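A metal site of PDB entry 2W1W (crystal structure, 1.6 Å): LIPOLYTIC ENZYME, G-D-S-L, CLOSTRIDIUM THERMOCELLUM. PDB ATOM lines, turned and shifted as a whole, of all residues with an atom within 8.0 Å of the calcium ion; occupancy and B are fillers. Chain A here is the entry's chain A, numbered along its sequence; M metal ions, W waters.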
ATOM      1  N   ILE A   6      15.366   4.601 -21.171  1.00  0.00           N
ATOM      2  CA  ILE A   6      14.221   5.059 -21.971  1.00  0.00           C
ATOM      3  C   ILE A   6      14.661   6.069 -23.032  1.00  0.00           C
ATOM      4  O   ILE A   6      15.321   7.093 -22.763  1.00  0.00           O
ATOM      5  CB  ILE A   6      13.030   5.587 -21.130  1.00  0.00           C
ATOM      6  CG1 ILE A   6      12.538   4.506 -20.167  1.00  0.00           C
ATOM      7  CG2 ILE A   6      11.846   5.946 -22.028  1.00  0.00           C
ATOM      8  CD1 ILE A   6      11.578   4.979 -19.084  1.00  0.00           C
ATOM      9  N   TYR A   7      14.312   5.725 -24.249  1.00  0.00           N
ATOM     10  CA  TYR A   7      14.542   6.521 -25.444  1.00  0.00           C
ATOM     11  C   TYR A   7      13.219   7.207 -25.752  1.00  0.00           C
ATOM     12  O   TYR A   7      12.272   6.594 -26.213  1.00  0.00           O
ATOM     13  CB  TYR A   7      15.065   5.636 -26.583  1.00  0.00           C
ATOM     14  CG  TYR A   7      16.449   5.149 -26.266  1.00  0.00           C
ATOM     15  CD1 TYR A   7      17.562   5.915 -26.592  1.00  0.00           C
ATOM     16  CD2 TYR A   7      16.643   3.981 -25.548  1.00  0.00           C
ATOM     17  CE1 TYR A   7      18.832   5.507 -26.265  1.00  0.00           C
ATOM     18  CE2 TYR A   7      17.907   3.573 -25.198  1.00  0.00           C
ATOM     19  CZ  TYR A   7      18.997   4.319 -25.552  1.00  0.00           C
ATOM     20  OH  TYR A   7      20.269   3.901 -25.191  1.00  0.00           O
ATOM     21  N   GLN A   8      13.176   8.494 -25.443  1.00  0.00           N
ATOM     22  CA  GLN A   8      11.925   9.264 -25.464  1.00  0.00           C
ATOM     23  C   GLN A   8      11.536   9.659 -26.880  1.00  0.00           C
ATOM     24  O   GLN A   8      12.364   9.947 -27.711  1.00  0.00           O
ATOM     25  CB  GLN A   8      12.047  10.530 -24.592  1.00  0.00           C
ATOM     26  CG  GLN A   8      12.648  10.322 -23.187  1.00  0.00           C
ATOM     27  CD  GLN A   8      11.697   9.707 -22.236  1.00  0.00           C
ATOM     28  OE1 GLN A   8      10.489   9.646 -22.501  1.00  0.00           O
ATOM     29  NE2 GLN A   8      12.234   9.210 -21.107  1.00  0.00           N
ATOM     30  N   ALA A   9      10.236   9.754 -27.118  1.00  0.00           N
ATOM     31  CA  ALA A   9       9.699  10.238 -28.397  1.00  0.00           C
ATOM     32  C   ALA A   9      10.303  11.548 -28.813  1.00  0.00           C
ATOM     33  O   ALA A   9      10.633  11.756 -29.963  1.00  0.00           O
ATOM     34  CB  ALA A   9       8.154  10.352 -28.359  1.00  0.00           C
ATOM     35  N   GLU A  10      10.425  12.429 -27.837  1.00  0.00           N
ATOM     36  CA  GLU A  10      10.924  13.798 -28.086  1.00  0.00           C
ATOM     37  C   GLU A  10      12.337  13.852 -28.668  1.00  0.00           C
ATOM     38  O   GLU A  10      12.743  14.857 -29.267  1.00  0.00           O
ATOM     39  CB  GLU A  10      10.758  14.718 -26.842  1.00  0.00           C
ATOM     40  CG  GLU A  10      11.351  14.200 -25.530  1.00  0.00           C
ATOM     41  CD  GLU A  10      10.317  13.452 -24.674  1.00  0.00           C
ATOM     42  OE1 GLU A  10       9.388  12.837 -25.279  1.00  0.00           O
ATOM     43  OE2 GLU A  10      10.410  13.471 -23.411  1.00  0.00           O
ATOM     44  N   ASP A  11      13.049  12.737 -28.515  1.00  0.00           N
ATOM     45  CA  ASP A  11      14.431  12.612 -28.947  1.00  0.00           C
ATOM     46  C   ASP A  11      14.609  11.759 -30.174  1.00  0.00           C
ATOM     47  O   ASP A  11      15.722  11.550 -30.644  1.00  0.00           O
ATOM     48  CB  ASP A  11      15.279  11.993 -27.804  1.00  0.00           C
ATOM     49  CG  ASP A  11      15.390  12.875 -26.597  1.00  0.00           C
ATOM     50  OD1 ASP A  11      15.535  14.109 -26.737  1.00  0.00           O
ATOM     51  OD2 ASP A  11      15.342  12.322 -25.484  1.00  0.00           O
ATOM     52  N   GLU A  20       3.519  14.644 -31.176  1.00  0.00           N
ATOM     53  CA  GLU A  20       2.131  15.012 -30.822  1.00  0.00           C
ATOM     54  C   GLU A  20       1.936  14.943 -29.293  1.00  0.00           C
ATOM     55  O   GLU A  20       2.629  14.158 -28.603  1.00  0.00           O
ATOM     56  CB  GLU A  20       1.203  13.993 -31.532  1.00  0.00           C
ATOM     57  CG  GLU A  20      -0.284  14.268 -31.572  1.00  0.00           C
ATOM     58  CD  GLU A  20      -1.014  13.287 -32.487  1.00  0.00           C
ATOM     59  OE1 GLU A  20      -1.916  12.555 -31.988  1.00  0.00           O
ATOM     60  OE2 GLU A  20      -0.674  13.243 -33.716  1.00  0.00           O
ATOM     61  N   GLY A  25      -1.933  10.504 -21.476  1.00  0.00           N
ATOM     62  CA  GLY A  25      -1.335   9.276 -20.908  1.00  0.00           C
ATOM     63  C   GLY A  25       0.063   8.932 -21.347  1.00  0.00           C
ATOM     64  O   GLY A  25       0.671   7.961 -20.865  1.00  0.00           O
ATOM     65  N   TYR A  26       0.561   9.708 -22.281  1.00  0.00           N
ATOM     66  CA  TYR A  26       1.972   9.628 -22.703  1.00  0.00           C
ATOM     67  C   TYR A  26       2.875  10.048 -21.555  1.00  0.00           C
ATOM     68  O   TYR A  26       2.468  10.720 -20.599  1.00  0.00           O
ATOM     69  CB  TYR A  26       2.266  10.449 -23.981  1.00  0.00           C
ATOM     70  CG  TYR A  26       2.063  11.952 -23.819  1.00  0.00           C
ATOM     71  CD1 TYR A  26       3.073  12.754 -23.314  1.00  0.00           C
ATOM     72  CD2 TYR A  26       0.845  12.537 -24.131  1.00  0.00           C
ATOM     73  CE1 TYR A  26       2.862  14.109 -23.119  1.00  0.00           C
ATOM     74  CE2 TYR A  26       0.619  13.878 -23.928  1.00  0.00           C
ATOM     75  CZ  TYR A  26       1.642  14.651 -23.423  1.00  0.00           C
ATOM     76  OH  TYR A  26       1.443  16.002 -23.224  1.00  0.00           O
ATOM     77  N   THR A  27       4.121   9.655 -21.662  1.00  0.00           N
ATOM     78  CA  THR A  27       5.143  10.074 -20.738  1.00  0.00           C
ATOM     79  C   THR A  27       6.141  10.941 -21.454  1.00  0.00           C
ATOM     80  O   THR A  27       6.189  11.009 -22.665  1.00  0.00           O
ATOM     81  CB  THR A  27       5.836   8.882 -20.073  1.00  0.00           C
ATOM     82  OG1 THR A  27       6.461   8.075 -21.065  1.00  0.00           O
ATOM     83  CG2 THR A  27       4.797   8.067 -19.258  1.00  0.00           C
ATOM     84  N   GLY A  28       6.995  11.564 -20.662  1.00  0.00           N
ATOM     85  CA  GLY A  28       7.834  12.623 -21.153  1.00  0.00           C
ATOM     86  C   GLY A  28       6.958  13.724 -21.729  1.00  0.00           C
ATOM     87  O   GLY A  28       5.812  13.958 -21.328  1.00  0.00           O
ATOM     88  N   SER A  29       7.499  14.355 -22.750  1.00  0.00           N
ATOM     89  CA  SER A  29       6.832  15.545 -23.318  1.00  0.00           C
ATOM     90  C   SER A  29       5.952  15.308 -24.533  1.00  0.00           C
ATOM     91  O   SER A  29       5.186  16.166 -24.957  1.00  0.00           O
ATOM     92  CB  SER A  29       7.885  16.550 -23.645  1.00  0.00           C
ATOM     93  OG  SER A  29       8.635  16.117 -24.733  1.00  0.00           O
ATOM     94  N   CYS A  30       6.029  14.114 -25.110  1.00  0.00           N
ATOM     95  CA  CYS A  30       5.238  13.837 -26.278  1.00  0.00           C
ATOM     96  C   CYS A  30       5.287  12.355 -26.609  1.00  0.00           C
ATOM     97  O   CYS A  30       5.967  11.548 -25.958  1.00  0.00           O
ATOM     98  CB  CYS A  30       5.759  14.652 -27.459  1.00  0.00           C
ATOM     99  SG  CYS A  30       7.314  14.095 -28.141  1.00  0.00           S
ATOM    100  N   TYR A  31       4.543  12.040 -27.640  1.00  0.00           N
ATOM    101  CA  TYR A  31       4.584  10.764 -28.357  1.00  0.00           C
ATOM    102  C   TYR A  31       4.703  11.029 -29.833  1.00  0.00           C
ATOM    103  O   TYR A  31       4.588  12.180 -30.255  1.00  0.00           O
ATOM    104  CB  TYR A  31       3.343   9.887 -28.024  1.00  0.00           C
ATOM    105  CG  TYR A  31       2.029  10.506 -28.420  1.00  0.00           C
ATOM    106  CD1 TYR A  31       1.497  10.337 -29.675  1.00  0.00           C
ATOM    107  CD2 TYR A  31       1.328  11.299 -27.510  1.00  0.00           C
ATOM    108  CE1 TYR A  31       0.265  10.937 -30.025  1.00  0.00           C
ATOM    109  CE2 TYR A  31       0.115  11.865 -27.834  1.00  0.00           C
ATOM    110  CZ  TYR A  31      -0.400  11.697 -29.092  1.00  0.00           C
ATOM    111  OH  TYR A  31      -1.603  12.295 -29.412  1.00  0.00           O
ATOM    112  N   VAL A  32       4.905   9.968 -30.597  1.00  0.00           N
ATOM    113  CA  VAL A  32       4.986  10.018 -32.054  1.00  0.00           C
ATOM    114  C   VAL A  32       3.747   9.418 -32.699  1.00  0.00           C
ATOM    115  O   VAL A  32       3.282   8.356 -32.290  1.00  0.00           O
ATOM    116  CB  VAL A  32       6.194   9.217 -32.596  1.00  0.00           C
ATOM    117  CG1 VAL A  32       6.261   9.311 -34.137  1.00  0.00           C
ATOM    118  CG2 VAL A  32       7.517   9.655 -31.902  1.00  0.00           C
ATOM    119  N   TRP A  44      16.007   5.644 -33.108  1.00  0.00           N
ATOM    120  CA  TRP A  44      16.909   6.179 -32.108  1.00  0.00           C
ATOM    121  C   TRP A  44      18.287   5.553 -32.264  1.00  0.00           C
ATOM    122  O   TRP A  44      18.462   4.479 -32.789  1.00  0.00           O
ATOM    123  CB  TRP A  44      16.431   5.829 -30.680  1.00  0.00           C
ATOM    124  CG  TRP A  44      15.165   6.479 -30.204  1.00  0.00           C
ATOM    125  CD1 TRP A  44      15.068   7.653 -29.501  1.00  0.00           C
ATOM    126  CD2 TRP A  44      13.829   5.973 -30.319  1.00  0.00           C
ATOM    127  NE1 TRP A  44      13.760   7.902 -29.194  1.00  0.00           N
ATOM    128  CE2 TRP A  44      12.981   6.886 -29.664  1.00  0.00           C
ATOM    129  CE3 TRP A  44      13.251   4.858 -30.932  1.00  0.00           C
ATOM    130  CZ2 TRP A  44      11.597   6.682 -29.558  1.00  0.00           C
ATOM    131  CZ3 TRP A  44      11.897   4.674 -30.821  1.00  0.00           C
ATOM    132  CH2 TRP A  44      11.091   5.579 -30.162  1.00  0.00           C
ATOM    133  N   ARG A  59       6.283   1.423 -25.664  1.00  0.00           N
ATOM    134  CA  ARG A  59       5.015   1.797 -25.070  1.00  0.00           C
ATOM    135  C   ARG A  59       4.235   2.556 -26.135  1.00  0.00           C
ATOM    136  O   ARG A  59       4.774   3.443 -26.777  1.00  0.00           O
ATOM    137  CB  ARG A  59       5.204   2.587 -23.765  1.00  0.00           C
ATOM    138  CG  ARG A  59       3.931   2.980 -23.050  1.00  0.00           C
ATOM    139  CD  ARG A  59       4.199   3.573 -21.644  1.00  0.00           C
ATOM    140  NE  ARG A  59       2.956   3.702 -20.851  1.00  0.00           N
ATOM    141  CZ  ARG A  59       2.187   4.784 -20.770  1.00  0.00           C
ATOM    142  NH1 ARG A  59       1.109   4.780 -19.987  1.00  0.00           N
ATOM    143  NH2 ARG A  59       2.499   5.867 -21.459  1.00  0.00           N
ATOM    144  N   TRP A  94      -2.623   3.114 -23.080  1.00  0.00           N
ATOM    145  CA  TRP A  94      -1.260   2.761 -23.492  1.00  0.00           C
ATOM    146  C   TRP A  94      -0.877   1.400 -22.968  1.00  0.00           C
ATOM    147  O   TRP A  94      -1.109   1.067 -21.804  1.00  0.00           O
ATOM    148  CB  TRP A  94      -0.271   3.823 -22.963  1.00  0.00           C
ATOM    149  CG  TRP A  94      -0.618   5.213 -23.416  1.00  0.00           C
ATOM    150  CD1 TRP A  94      -1.532   6.053 -22.842  1.00  0.00           C
ATOM    151  CD2 TRP A  94      -0.046   5.923 -24.525  1.00  0.00           C
ATOM    152  NE1 TRP A  94      -1.565   7.246 -23.546  1.00  0.00           N
ATOM    153  CE2 TRP A  94      -0.665   7.179 -24.583  1.00  0.00           C
ATOM    154  CE3 TRP A  94       0.929   5.603 -25.493  1.00  0.00           C
ATOM    155  CZ2 TRP A  94      -0.347   8.100 -25.576  1.00  0.00           C
ATOM    156  CZ3 TRP A  94       1.249   6.513 -26.452  1.00  0.00           C
ATOM    157  CH2 TRP A  94       0.604   7.746 -26.501  1.00  0.00           C
ATOM    158  N   VAL A 123       3.427   6.049 -30.567  1.00  0.00           N
ATOM    159  CA  VAL A 123       4.535   5.455 -29.755  1.00  0.00           C
ATOM    160  C   VAL A 123       5.060   6.489 -28.764  1.00  0.00           C
ATOM    161  O   VAL A 123       5.470   7.593 -29.117  1.00  0.00           O
ATOM    162  CB  VAL A 123       5.690   4.934 -30.653  1.00  0.00           C
ATOM    163  CG1 VAL A 123       6.889   4.447 -29.804  1.00  0.00           C
ATOM    164  CG2 VAL A 123       5.233   3.831 -31.562  1.00  0.00           C
ATOM    165  N   ASP A 124       5.009   6.080 -27.513  1.00  0.00           N
ATOM    166  CA  ASP A 124       5.418   6.896 -26.368  1.00  0.00           C
ATOM    167  C   ASP A 124       6.948   6.969 -26.229  1.00  0.00           C
ATOM    168  O   ASP A 124       7.527   8.041 -26.051  1.00  0.00           O
ATOM    169  CB  ASP A 124       4.798   6.346 -25.080  1.00  0.00           C
ATOM    170  CG  ASP A 124       4.893   7.281 -23.911  1.00  0.00           C
ATOM    171  OD1 ASP A 124       5.072   8.515 -24.087  1.00  0.00           O
ATOM    172  OD2 ASP A 124       4.815   6.735 -22.768  1.00  0.00           O
ATOM    173  N   TYR A 125       7.553   5.789 -26.271  1.00  0.00           N
ATOM    174  CA  TYR A 125       8.999   5.625 -26.114  1.00  0.00           C
ATOM    175  C   TYR A 125       9.390   4.217 -26.483  1.00  0.00           C
ATOM    176  O   TYR A 125       8.554   3.350 -26.648  1.00  0.00           O
ATOM    177  CB  TYR A 125       9.446   5.899 -24.674  1.00  0.00           C
ATOM    178  CG  TYR A 125       8.833   5.045 -23.576  1.00  0.00           C
ATOM    179  CD1 TYR A 125       9.054   3.678 -23.496  1.00  0.00           C
ATOM    180  CD2 TYR A 125       8.095   5.629 -22.557  1.00  0.00           C
ATOM    181  CE1 TYR A 125       8.581   2.917 -22.440  1.00  0.00           C
ATOM    182  CE2 TYR A 125       7.592   4.872 -21.502  1.00  0.00           C
ATOM    183  CZ  TYR A 125       7.828   3.506 -21.469  1.00  0.00           C
ATOM    184  OH  TYR A 125       7.325   2.723 -20.448  1.00  0.00           O
ATOM    185  N   LEU A 126      10.705   4.059 -26.590  1.00  0.00           N
ATOM    186  CA  LEU A 126      11.383   2.763 -26.625  1.00  0.00           C
ATOM    187  C   LEU A 126      12.216   2.628 -25.337  1.00  0.00           C
ATOM    188  O   LEU A 126      13.002   3.484 -24.987  1.00  0.00           O
ATOM    189  CB  LEU A 126      12.310   2.682 -27.825  1.00  0.00           C
ATOM    190  CG  LEU A 126      13.344   1.550 -27.863  1.00  0.00           C
ATOM    191  CD1 LEU A 126      12.674   0.165 -27.932  1.00  0.00           C
ATOM    192  CD2 LEU A 126      14.369   1.750 -29.025  1.00  0.00           C
HETATM  193 CA    CA M   1       6.745   9.959 -24.635  1.00  0.00          CA
HETATM  194  O   HOH W   1       8.870  10.104 -24.280  1.00  0.00           O
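Water W1 binds the calcium ion (2.2 Å).
O of Cys 30 is bound to the calcium ion.
The calcium ion is bound by the side-chain carboxylate (OD1) of Asp 124, at 2.3 Å.
The calcium ion is bound by O of Thr 27 (2.3 Å).
The calcium ion is bound by the backbone carbonyl oxygen (O) of Asp 124.
The side-chain sulfur (SG) of Cys 30 sits at hydrogen-bond distance from the backbone NH (N) of Glu 10, 3.5 Å away.
The backbone carbonyl oxygen (O) of Asp 124 sits close to the backbone NH (N) of Ala 9.
The guanidinium group (NH2) of Arg 59 is in salt-bridge range of the side-chain carboxylate (OD2) of Asp 124, at 2.8 Å.
The backbone NH (N) of Ser 29 lies within hydrogen-bond range of the side-chain carboxylate (OE2) of Glu 10 (3.1 Å).
Residues that only touch the calcium ion: Glu 10 (3.96 Å).
Within 4 Å of the calcium ion: Glu 10, Thr 27, Cys 30 and Asp 124.
The nearest printed residue that does not touch the calcium ion is Ala 9 (4.001 Å).
Water W1 lies within hydrogen-bond range of the side-chain amide oxygen (OE1) of Gln 8, the side-chain carboxylate (OE1) of Glu 10 and the backbone NH (N) of Ala 9.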
